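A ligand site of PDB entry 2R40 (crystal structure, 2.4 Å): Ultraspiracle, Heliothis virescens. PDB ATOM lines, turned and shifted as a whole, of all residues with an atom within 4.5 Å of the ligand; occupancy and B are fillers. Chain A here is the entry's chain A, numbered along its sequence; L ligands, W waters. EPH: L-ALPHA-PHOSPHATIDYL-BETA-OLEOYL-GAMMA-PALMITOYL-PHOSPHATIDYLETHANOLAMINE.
The backbone carbonyl oxygen of Gln 135 sits at hydrogen-bond distance from a nitrogen (N1) of the ligand.
A nitrogen (N1) of the ligand lies close to the backbone NH (N) of Gly 137, 3.2 Å away.
ND2 of Asn 84 sits at hydrogen-bond distance from OG of Ser 228, 3.2 Å away.
The backbone NH (N) of Val 138 is in hydrogen-bond range of the backbone carbonyl oxygen (O) of Ala 133, at 2.7 Å.
O of Met 120 sits at hydrogen-bond distance from N of Leu 128, at 2.8 Å.
The backbone carbonyl oxygen (O) of Leu 232 is in hydrogen-bond range of the backbone NH (N) of Leu 237 (2.8 Å).
The backbone carbonyl oxygen (O) of Val 43 is in hydrogen-bond range of the side-chain sulfur (SG) of Cys 47, at 3.2 Å.
Merely in contact with the ligand: Val 35, Pro 36, Phe 39, Val 43, Leu 46, Asn 84, Leu 87, Leu 88, Met 120, Leu 128, Ser 132, Ala 136, Val 138, Phe 142, Ser 228, His 231, Leu 232, Phe 235 and Leu 237.
Of the 29 residues printed, 21 come within 4 Å of the ligand.
The nearest printed residue that does not touch the ligand is Ala 133 (4.02 Å).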
ATOM      1  N   LEU A  27     -10.473  -3.774  15.888  1.00  0.00           N
ATOM      2  CA  LEU A  27     -11.666  -4.473  15.445  1.00  0.00           C
ATOM      3  C   LEU A  27     -12.159  -3.872  14.135  1.00  0.00           C
ATOM      4  O   LEU A  27     -12.161  -2.655  13.965  1.00  0.00           O
ATOM      5  CB  LEU A  27     -12.753  -4.386  16.512  1.00  0.00           C
ATOM      6  CG  LEU A  27     -12.339  -4.734  17.943  1.00  0.00           C
ATOM      7  CD1 LEU A  27     -13.372  -4.279  18.974  1.00  0.00           C
ATOM      8  CD2 LEU A  27     -12.062  -6.228  18.075  1.00  0.00           C
ATOM      9  N   VAL A  35     -19.667 -12.495   8.226  1.00  0.00           N
ATOM     10  CA  VAL A  35     -20.833 -11.694   8.611  1.00  0.00           C
ATOM     11  C   VAL A  35     -21.695 -11.442   7.372  1.00  0.00           C
ATOM     12  O   VAL A  35     -21.179 -10.980   6.357  1.00  0.00           O
ATOM     13  CB  VAL A  35     -20.406 -10.336   9.276  1.00  0.00           C
ATOM     14  CG1 VAL A  35     -21.602  -9.407   9.468  1.00  0.00           C
ATOM     15  CG2 VAL A  35     -19.701 -10.570  10.618  1.00  0.00           C
ATOM     16  N   PRO A  36     -23.007 -11.754   7.445  1.00  0.00           N
ATOM     17  CA  PRO A  36     -23.922 -11.549   6.329  1.00  0.00           C
ATOM     18  C   PRO A  36     -23.986 -10.077   5.931  1.00  0.00           C
ATOM     19  O   PRO A  36     -23.880  -9.216   6.805  1.00  0.00           O
ATOM     20  CB  PRO A  36     -25.282 -11.975   6.896  1.00  0.00           C
ATOM     21  CG  PRO A  36     -24.980 -12.839   8.012  1.00  0.00           C
ATOM     22  CD  PRO A  36     -23.703 -12.335   8.610  1.00  0.00           C
ATOM     23  N   PHE A  39     -26.022  -7.436   7.917  1.00  0.00           N
ATOM     24  CA  PHE A  39     -25.517  -7.098   9.248  1.00  0.00           C
ATOM     25  C   PHE A  39     -24.075  -6.574   9.291  1.00  0.00           C
ATOM     26  O   PHE A  39     -23.507  -6.463  10.366  1.00  0.00           O
ATOM     27  CB  PHE A  39     -25.675  -8.283  10.216  1.00  0.00           C
ATOM     28  CG  PHE A  39     -27.098  -8.710  10.422  1.00  0.00           C
ATOM     29  CD1 PHE A  39     -27.972  -7.945  11.187  1.00  0.00           C
ATOM     30  CD2 PHE A  39     -27.576  -9.896   9.853  1.00  0.00           C
ATOM     31  CE1 PHE A  39     -29.299  -8.339  11.391  1.00  0.00           C
ATOM     32  CE2 PHE A  39     -28.901 -10.304  10.037  1.00  0.00           C
ATOM     33  CZ  PHE A  39     -29.763  -9.519  10.810  1.00  0.00           C
ATOM     34  N   PRO A  42     -24.243  -2.667  11.133  1.00  0.00           N
ATOM     35  CA  PRO A  42     -24.280  -2.737  12.596  1.00  0.00           C
ATOM     36  C   PRO A  42     -23.002  -3.247  13.244  1.00  0.00           C
ATOM     37  O   PRO A  42     -22.540  -2.643  14.200  1.00  0.00           O
ATOM     38  CB  PRO A  42     -25.428  -3.706  12.866  1.00  0.00           C
ATOM     39  CG  PRO A  42     -26.298  -3.571  11.734  1.00  0.00           C
ATOM     40  CD  PRO A  42     -25.417  -3.342  10.548  1.00  0.00           C
ATOM     41  N   VAL A  43     -22.459  -4.355  12.742  1.00  0.00           N
ATOM     42  CA  VAL A  43     -21.227  -4.945  13.280  1.00  0.00           C
ATOM     43  C   VAL A  43     -20.001  -4.035  13.084  1.00  0.00           C
ATOM     44  O   VAL A  43     -19.173  -3.892  13.977  1.00  0.00           O
ATOM     45  CB  VAL A  43     -21.005  -6.398  12.698  1.00  0.00           C
ATOM     46  CG1 VAL A  43     -19.707  -7.023  13.213  1.00  0.00           C
ATOM     47  CG2 VAL A  43     -22.197  -7.298  13.050  1.00  0.00           C
ATOM     48  N   LEU A  46     -20.228  -1.379  15.621  1.00  0.00           N
ATOM     49  CA  LEU A  46     -19.831  -1.895  16.945  1.00  0.00           C
ATOM     50  C   LEU A  46     -18.328  -2.071  17.077  1.00  0.00           C
ATOM     51  O   LEU A  46     -17.760  -1.867  18.154  1.00  0.00           O
ATOM     52  CB  LEU A  46     -20.560  -3.205  17.276  1.00  0.00           C
ATOM     53  CG  LEU A  46     -22.099  -3.121  17.359  1.00  0.00           C
ATOM     54  CD1 LEU A  46     -22.718  -4.442  17.794  1.00  0.00           C
ATOM     55  CD2 LEU A  46     -22.562  -1.982  18.274  1.00  0.00           C
ATOM     56  N   CYS A  47     -17.689  -2.455  15.971  1.00  0.00           N
ATOM     57  CA  CYS A  47     -16.226  -2.524  15.889  1.00  0.00           C
ATOM     58  C   CYS A  47     -15.579  -1.158  16.151  1.00  0.00           C
ATOM     59  O   CYS A  47     -14.599  -1.054  16.892  1.00  0.00           O
ATOM     60  CB  CYS A  47     -15.806  -3.113  14.537  1.00  0.00           C
ATOM     61  SG  CYS A  47     -16.169  -4.906  14.377  1.00  0.00           S
ATOM     62  N   ASN A  84      -8.829  -6.992  25.946  1.00  0.00           N
ATOM     63  CA  ASN A  84     -10.105  -7.701  25.821  1.00  0.00           C
ATOM     64  C   ASN A  84     -10.771  -7.868  27.187  1.00  0.00           C
ATOM     65  O   ASN A  84     -11.941  -7.543  27.336  1.00  0.00           O
ATOM     66  CB  ASN A  84      -9.943  -9.038  25.084  1.00  0.00           C
ATOM     67  CG  ASN A  84     -11.282  -9.681  24.729  1.00  0.00           C
ATOM     68  OD1 ASN A  84     -11.793  -9.526  23.632  1.00  0.00           O
ATOM     69  ND2 ASN A  84     -11.866 -10.372  25.676  1.00  0.00           N
ATOM     70  N   LEU A  87     -11.986  -4.383  28.385  1.00  0.00           N
ATOM     71  CA  LEU A  87     -13.214  -3.957  27.685  1.00  0.00           C
ATOM     72  C   LEU A  87     -14.454  -4.643  28.238  1.00  0.00           C
ATOM     73  O   LEU A  87     -15.493  -4.003  28.396  1.00  0.00           O
ATOM     74  CB  LEU A  87     -13.128  -4.261  26.197  1.00  0.00           C
ATOM     75  CG  LEU A  87     -12.584  -3.350  25.093  1.00  0.00           C
ATOM     76  CD1 LEU A  87     -13.299  -3.804  23.815  1.00  0.00           C
ATOM     77  CD2 LEU A  87     -12.855  -1.899  25.331  1.00  0.00           C
ATOM     78  N   LEU A  88     -14.367  -5.948  28.493  1.00  0.00           N
ATOM     79  CA  LEU A  88     -15.497  -6.700  29.025  1.00  0.00           C
ATOM     80  C   LEU A  88     -15.804  -6.313  30.465  1.00  0.00           C
ATOM     81  O   LEU A  88     -16.971  -6.179  30.871  1.00  0.00           O
ATOM     82  CB  LEU A  88     -15.272  -8.208  28.899  1.00  0.00           C
ATOM     83  CG  LEU A  88     -15.468  -8.818  27.506  1.00  0.00           C
ATOM     84  CD1 LEU A  88     -14.804 -10.183  27.442  1.00  0.00           C
ATOM     85  CD2 LEU A  88     -16.949  -8.926  27.122  1.00  0.00           C
ATOM     86  N   ILE A  91     -17.666  -3.027  30.322  1.00  0.00           N
ATOM     87  CA  ILE A  91     -19.036  -3.322  29.903  1.00  0.00           C
ATOM     88  C   ILE A  91     -19.898  -3.824  31.080  1.00  0.00           C
ATOM     89  O   ILE A  91     -21.058  -3.447  31.220  1.00  0.00           O
ATOM     90  CB  ILE A  91     -19.051  -4.384  28.755  1.00  0.00           C
ATOM     91  CG1 ILE A  91     -18.528  -3.778  27.438  1.00  0.00           C
ATOM     92  CG2 ILE A  91     -20.438  -4.957  28.574  1.00  0.00           C
ATOM     93  CD1 ILE A  91     -18.281  -4.783  26.329  1.00  0.00           C
ATOM     94  N   MET A 120     -27.106  -4.827  27.845  1.00  0.00           N
ATOM     95  CA  MET A 120     -25.669  -4.717  28.035  1.00  0.00           C
ATOM     96  C   MET A 120     -25.220  -3.335  27.582  1.00  0.00           C
ATOM     97  O   MET A 120     -25.371  -2.978  26.408  1.00  0.00           O
ATOM     98  CB  MET A 120     -24.955  -5.847  27.268  1.00  0.00           C
ATOM     99  CG  MET A 120     -23.479  -5.663  27.107  1.00  0.00           C
ATOM    100  SD  MET A 120     -22.658  -7.079  26.361  1.00  0.00           S
ATOM    101  CE  MET A 120     -22.968  -8.376  27.563  1.00  0.00           C
ATOM    102  N   LEU A 122     -22.837  -1.069  26.188  1.00  0.00           N
ATOM    103  CA  LEU A 122     -21.619  -1.008  25.413  1.00  0.00           C
ATOM    104  C   LEU A 122     -20.847   0.273  25.629  1.00  0.00           C
ATOM    105  O   LEU A 122     -19.633   0.281  25.560  1.00  0.00           O
ATOM    106  CB  LEU A 122     -21.918  -1.201  23.927  1.00  0.00           C
ATOM    107  CG  LEU A 122     -21.394  -2.508  23.348  1.00  0.00           C
ATOM    108  CD1 LEU A 122     -21.996  -3.743  24.039  1.00  0.00           C
ATOM    109  CD2 LEU A 122     -21.620  -2.543  21.835  1.00  0.00           C
ATOM    110  N   LEU A 128     -27.040  -2.928  24.190  1.00  0.00           N
ATOM    111  CA  LEU A 128     -27.190  -4.072  23.327  1.00  0.00           C
ATOM    112  C   LEU A 128     -28.243  -4.947  23.980  1.00  0.00           C
ATOM    113  O   LEU A 128     -28.141  -5.283  25.173  1.00  0.00           O
ATOM    114  CB  LEU A 128     -25.870  -4.835  23.266  1.00  0.00           C
ATOM    115  CG  LEU A 128     -25.417  -5.564  22.007  1.00  0.00           C
ATOM    116  CD1 LEU A 128     -24.168  -6.350  22.367  1.00  0.00           C
ATOM    117  CD2 LEU A 128     -26.480  -6.509  21.457  1.00  0.00           C
ATOM    118  N   SER A 132     -30.681  -9.634  20.279  1.00  0.00           N
ATOM    119  CA  SER A 132     -29.701  -9.404  19.238  1.00  0.00           C
ATOM    120  C   SER A 132     -28.477 -10.291  19.421  1.00  0.00           C
ATOM    121  O   SER A 132     -27.909 -10.757  18.430  1.00  0.00           O
ATOM    122  CB  SER A 132     -29.291  -7.939  19.234  1.00  0.00           C
ATOM    123  OG  SER A 132     -30.445  -7.115  19.131  1.00  0.00           O
ATOM    124  N   ALA A 133     -28.059 -10.500  20.672  1.00  0.00           N
ATOM    125  CA  ALA A 133     -27.004 -11.453  20.996  1.00  0.00           C
ATOM    126  C   ALA A 133     -27.437 -12.854  20.606  1.00  0.00           C
ATOM    127  O   ALA A 133     -26.633 -13.635  20.075  1.00  0.00           O
ATOM    128  CB  ALA A 133     -26.652 -11.408  22.464  1.00  0.00           C
ATOM    129  N   LEU A 134     -28.700 -13.176  20.874  1.00  0.00           N
ATOM    130  CA  LEU A 134     -29.315 -14.423  20.437  1.00  0.00           C
ATOM    131  C   LEU A 134     -29.264 -14.578  18.905  1.00  0.00           C
ATOM    132  O   LEU A 134     -28.746 -15.581  18.413  1.00  0.00           O
ATOM    133  CB  LEU A 134     -30.753 -14.550  20.958  1.00  0.00           C
ATOM    134  CG  LEU A 134     -30.940 -14.687  22.487  1.00  0.00           C
ATOM    135  CD1 LEU A 134     -32.410 -14.598  22.861  1.00  0.00           C
ATOM    136  CD2 LEU A 134     -30.325 -15.972  23.034  1.00  0.00           C
ATOM    137  N   GLN A 135     -29.778 -13.581  18.163  1.00  0.00           N
ATOM    138  CA  GLN A 135     -29.639 -13.543  16.704  1.00  0.00           C
ATOM    139  C   GLN A 135     -28.206 -13.786  16.241  1.00  0.00           C
ATOM    140  O   GLN A 135     -27.974 -14.579  15.338  1.00  0.00           O
ATOM    141  CB  GLN A 135     -30.151 -12.215  16.121  1.00  0.00           C
ATOM    142  CG  GLN A 135     -31.662 -12.104  15.977  1.00  0.00           C
ATOM    143  CD  GLN A 135     -32.100 -10.801  15.321  1.00  0.00           C
ATOM    144  OE1 GLN A 135     -31.765 -10.516  14.166  1.00  0.00           O
ATOM    145  NE2 GLN A 135     -32.889 -10.003  16.054  1.00  0.00           N
ATOM    146  N   ALA A 136     -27.242 -13.121  16.886  1.00  0.00           N
ATOM    147  CA  ALA A 136     -25.832 -13.253  16.534  1.00  0.00           C
ATOM    148  C   ALA A 136     -25.166 -14.522  17.067  1.00  0.00           C
ATOM    149  O   ALA A 136     -23.956 -14.726  16.867  1.00  0.00           O
ATOM    150  CB  ALA A 136     -25.044 -12.031  16.979  1.00  0.00           C
ATOM    151  N   GLY A 137     -25.938 -15.369  17.735  1.00  0.00           N
ATOM    152  CA  GLY A 137     -25.418 -16.607  18.342  1.00  0.00           C
ATOM    153  C   GLY A 137     -24.464 -16.451  19.513  1.00  0.00           C
ATOM    154  O   GLY A 137     -23.718 -17.389  19.830  1.00  0.00           O
ATOM    155  N   VAL A 138     -24.465 -15.290  20.164  1.00  0.00           N
ATOM    156  CA  VAL A 138     -23.599 -15.046  21.330  1.00  0.00           C
ATOM    157  C   VAL A 138     -24.391 -14.862  22.640  1.00  0.00           C
ATOM    158  O   VAL A 138     -23.943 -14.169  23.544  1.00  0.00           O
ATOM    159  CB  VAL A 138     -22.623 -13.832  21.102  1.00  0.00           C
ATOM    160  CG1 VAL A 138     -21.657 -14.118  19.971  1.00  0.00           C
ATOM    161  CG2 VAL A 138     -23.393 -12.544  20.782  1.00  0.00           C
ATOM    162  N   ILE A 141     -22.654 -16.203  26.157  1.00  0.00           N
ATOM    163  CA  ILE A 141     -21.625 -15.300  26.647  1.00  0.00           C
ATOM    164  C   ILE A 141     -22.181 -13.954  27.146  1.00  0.00           C
ATOM    165  O   ILE A 141     -21.683 -13.397  28.117  1.00  0.00           O
ATOM    166  CB  ILE A 141     -20.536 -15.093  25.575  1.00  0.00           C
ATOM    167  CG1 ILE A 141     -19.323 -14.416  26.174  1.00  0.00           C
ATOM    168  CG2 ILE A 141     -21.068 -14.311  24.363  1.00  0.00           C
ATOM    169  CD1 ILE A 141     -18.059 -14.880  25.547  1.00  0.00           C
ATOM    170  N   PHE A 142     -23.207 -13.452  26.460  1.00  0.00           N
ATOM    171  CA  PHE A 142     -23.923 -12.243  26.849  1.00  0.00           C
ATOM    172  C   PHE A 142     -24.443 -12.443  28.270  1.00  0.00           C
ATOM    173  O   PHE A 142     -24.240 -11.574  29.131  1.00  0.00           O
ATOM    174  CB  PHE A 142     -25.087 -12.025  25.857  1.00  0.00           C
ATOM    175  CG  PHE A 142     -25.944 -10.824  26.131  1.00  0.00           C
ATOM    176  CD1 PHE A 142     -26.990 -10.891  27.035  1.00  0.00           C
ATOM    177  CD2 PHE A 142     -25.753  -9.636  25.426  1.00  0.00           C
ATOM    178  CE1 PHE A 142     -27.811  -9.768  27.276  1.00  0.00           C
ATOM    179  CE2 PHE A 142     -26.567  -8.522  25.654  1.00  0.00           C
ATOM    180  CZ  PHE A 142     -27.593  -8.598  26.577  1.00  0.00           C
ATOM    181  N   SER A 228     -14.941 -14.942  24.197  1.00  0.00           N
ATOM    182  CA  SER A 228     -15.261 -13.858  23.272  1.00  0.00           C
ATOM    183  C   SER A 228     -14.278 -13.717  22.109  1.00  0.00           C
ATOM    184  O   SER A 228     -14.661 -13.322  21.010  1.00  0.00           O
ATOM    185  CB  SER A 228     -15.446 -12.543  24.035  1.00  0.00           C
ATOM    186  OG  SER A 228     -14.210 -11.866  24.178  1.00  0.00           O
ATOM    187  N   HIS A 231     -15.304 -16.267  19.384  1.00  0.00           N
ATOM    188  CA  HIS A 231     -16.358 -15.689  18.546  1.00  0.00           C
ATOM    189  C   HIS A 231     -15.811 -14.636  17.584  1.00  0.00           C
ATOM    190  O   HIS A 231     -16.078 -14.681  16.388  1.00  0.00           O
ATOM    191  CB  HIS A 231     -17.493 -15.101  19.401  1.00  0.00           C
ATOM    192  CG  HIS A 231     -18.306 -16.118  20.109  1.00  0.00           C
ATOM    193  ND1 HIS A 231     -17.995 -16.565  21.372  1.00  0.00           N
ATOM    194  CD2 HIS A 231     -19.404 -16.809  19.731  1.00  0.00           C
ATOM    195  CE1 HIS A 231     -18.875 -17.488  21.747  1.00  0.00           C
ATOM    196  NE2 HIS A 231     -19.739 -17.653  20.771  1.00  0.00           N
ATOM    197  N   LEU A 232     -15.003 -13.707  18.108  1.00  0.00           N
ATOM    198  CA  LEU A 232     -14.356 -12.660  17.321  1.00  0.00           C
ATOM    199  C   LEU A 232     -13.514 -13.170  16.141  1.00  0.00           C
ATOM    200  O   LEU A 232     -13.564 -12.598  15.049  1.00  0.00           O
ATOM    201  CB  LEU A 232     -13.489 -11.766  18.216  1.00  0.00           C
ATOM    202  CG  LEU A 232     -14.130 -10.770  19.191  1.00  0.00           C
ATOM    203  CD1 LEU A 232     -13.075 -10.190  20.136  1.00  0.00           C
ATOM    204  CD2 LEU A 232     -14.920  -9.653  18.468  1.00  0.00           C
ATOM    205  N   PHE A 235     -15.685 -14.805  13.338  1.00  0.00           N
ATOM    206  CA  PHE A 235     -16.272 -13.819  12.427  1.00  0.00           C
ATOM    207  C   PHE A 235     -15.239 -12.910  11.768  1.00  0.00           C
ATOM    208  O   PHE A 235     -15.589 -11.978  11.036  1.00  0.00           O
ATOM    209  CB  PHE A 235     -17.365 -13.021  13.118  1.00  0.00           C
ATOM    210  CG  PHE A 235     -18.564 -13.837  13.506  1.00  0.00           C
ATOM    211  CD1 PHE A 235     -19.489 -14.246  12.557  1.00  0.00           C
ATOM    212  CD2 PHE A 235     -18.768 -14.192  14.838  1.00  0.00           C
ATOM    213  CE1 PHE A 235     -20.595 -15.002  12.907  1.00  0.00           C
ATOM    214  CE2 PHE A 235     -19.878 -14.959  15.209  1.00  0.00           C
ATOM    215  CZ  PHE A 235     -20.792 -15.354  14.232  1.00  0.00           C
ATOM    216  N   LEU A 237     -13.156 -10.671  13.019  1.00  0.00           N
ATOM    217  CA  LEU A 237     -13.366  -9.298  13.494  1.00  0.00           C
ATOM    218  C   LEU A 237     -12.137  -8.666  14.119  1.00  0.00           C
ATOM    219  O   LEU A 237     -12.121  -7.466  14.362  1.00  0.00           O
ATOM    220  CB  LEU A 237     -14.537  -9.262  14.486  1.00  0.00           C
ATOM    221  CG  LEU A 237     -15.971  -8.906  14.045  1.00  0.00           C
ATOM    222  CD1 LEU A 237     -16.256  -9.023  12.535  1.00  0.00           C
ATOM    223  CD2 LEU A 237     -16.999  -9.692  14.868  1.00  0.00           C
HETATM  224  C1  EPH L   1     -26.846 -10.966  13.821  1.00  0.00           C
HETATM  225  C2  EPH L   1     -25.890 -11.665  12.865  1.00  0.00           C
HETATM  226  C4  EPH L   1     -27.019  -8.737  14.592  1.00  0.00           C
HETATM  227  O2  EPH L   1     -26.573  -9.579  13.619  1.00  0.00           O
HETATM  228  O4  EPH L   1     -28.038  -8.985  15.225  1.00  0.00           O
HETATM  229  C18 EPH L   1     -26.191  -7.462  14.854  1.00  0.00           C
HETATM  230  C19 EPH L   1     -25.933  -7.245  16.353  1.00  0.00           C
HETATM  231  C20 EPH L   1     -24.938  -8.255  16.915  1.00  0.00           C
HETATM  232  C21 EPH L   1     -24.976  -8.256  18.445  1.00  0.00           C
HETATM  233  C22 EPH L   1     -23.783  -9.025  19.039  1.00  0.00           C
HETATM  234  C23 EPH L   1     -22.598  -8.120  19.403  1.00  0.00           C
HETATM  235  C24 EPH L   1     -21.626  -7.955  18.208  1.00  0.00           C
HETATM  236  C25 EPH L   1     -20.193  -7.706  18.690  1.00  0.00           C
HETATM  237  C26 EPH L   1     -19.398  -6.799  17.727  1.00  0.00           C
HETATM  238  C27 EPH L   1     -18.327  -5.973  18.466  1.00  0.00           C
HETATM  239  C28 EPH L   1     -18.885  -5.412  19.790  1.00  0.00           C
HETATM  240  C29 EPH L   1     -18.025  -4.292  20.360  1.00  0.00           C
HETATM  241  C30 EPH L   1     -17.633  -4.555  21.811  1.00  0.00           C
HETATM  242  C31 EPH L   1     -16.269  -5.256  21.897  1.00  0.00           C
HETATM  243  C32 EPH L   1     -16.204  -6.174  23.114  1.00  0.00           C
HETATM  244  C33 EPH L   1     -15.256  -7.353  22.862  1.00  0.00           C
HETATM  245  C34 EPH L   1     -14.506  -7.726  24.133  1.00  0.00           C
HETATM  246  C37 EPH L   1     -26.550 -12.923  12.306  1.00  0.00           C
HETATM  247  O5  EPH L   1     -25.624 -13.603  11.437  1.00  0.00           O
HETATM  248  C3  EPH L   1     -23.480 -11.751  12.908  1.00  0.00           C
HETATM  249  O1  EPH L   1     -24.662 -12.009  13.559  1.00  0.00           O
HETATM  250  O3  EPH L   1     -23.446 -11.536  11.695  1.00  0.00           O
HETATM  251  C5  EPH L   1     -22.186 -11.734  13.705  1.00  0.00           C
HETATM  252  C6  EPH L   1     -22.249 -10.688  14.821  1.00  0.00           C
HETATM  253  C7  EPH L   1     -20.890 -10.503  15.474  1.00  0.00           C
HETATM  254  C8  EPH L   1     -20.820 -11.286  16.783  1.00  0.00           C
HETATM  255  C9  EPH L   1     -19.432 -11.133  17.422  1.00  0.00           C
HETATM  256  C10 EPH L   1     -19.515 -11.353  18.930  1.00  0.00           C
HETATM  257  C11 EPH L   1     -18.134 -11.587  19.520  1.00  0.00           C
HETATM  258  C12 EPH L   1     -17.894 -10.730  20.753  1.00  0.00           C
HETATM  259  C13 EPH L   1     -18.552 -11.334  21.998  1.00  0.00           C
HETATM  260  C14 EPH L   1     -18.236 -10.511  23.253  1.00  0.00           C
HETATM  261  C15 EPH L   1     -18.514  -9.016  23.056  1.00  0.00           C
HETATM  262  C16 EPH L   1     -19.593  -8.497  24.004  1.00  0.00           C
HETATM  263  C17 EPH L   1     -20.984  -8.781  23.438  1.00  0.00           C
HETATM  264  C35 EPH L   1     -21.636  -9.945  24.174  1.00  0.00           C
HETATM  265  C36 EPH L   1     -22.898 -10.367  23.444  1.00  0.00           C
HETATM  266  P1  EPH L   1     -25.638 -15.207  11.228  1.00  0.00           P
HETATM  267  O6  EPH L   1     -24.472 -15.544  10.361  1.00  0.00           O
HETATM  268  O7  EPH L   1     -27.004 -15.649  10.833  1.00  0.00           O
HETATM  269  O8  EPH L   1     -25.328 -15.756  12.741  1.00  0.00           O
HETATM  270  C38 EPH L   1     -25.131 -17.159  13.005  1.00  0.00           C
HETATM  271  C39 EPH L   1     -26.327 -17.734  13.795  1.00  0.00           C
HETATM  272  N1  EPH L   1     -26.550 -16.953  15.023  1.00  0.00           N
HETATM  273  O   HOH W   1     -22.790 -19.295  11.646  1.00  0.00           O
HETATM  274  O   HOH W   2     -29.560 -14.410  10.693  1.00  0.00           O
HETATM  275  O   HOH W   3     -21.931 -16.558   9.767  1.00  0.00           O
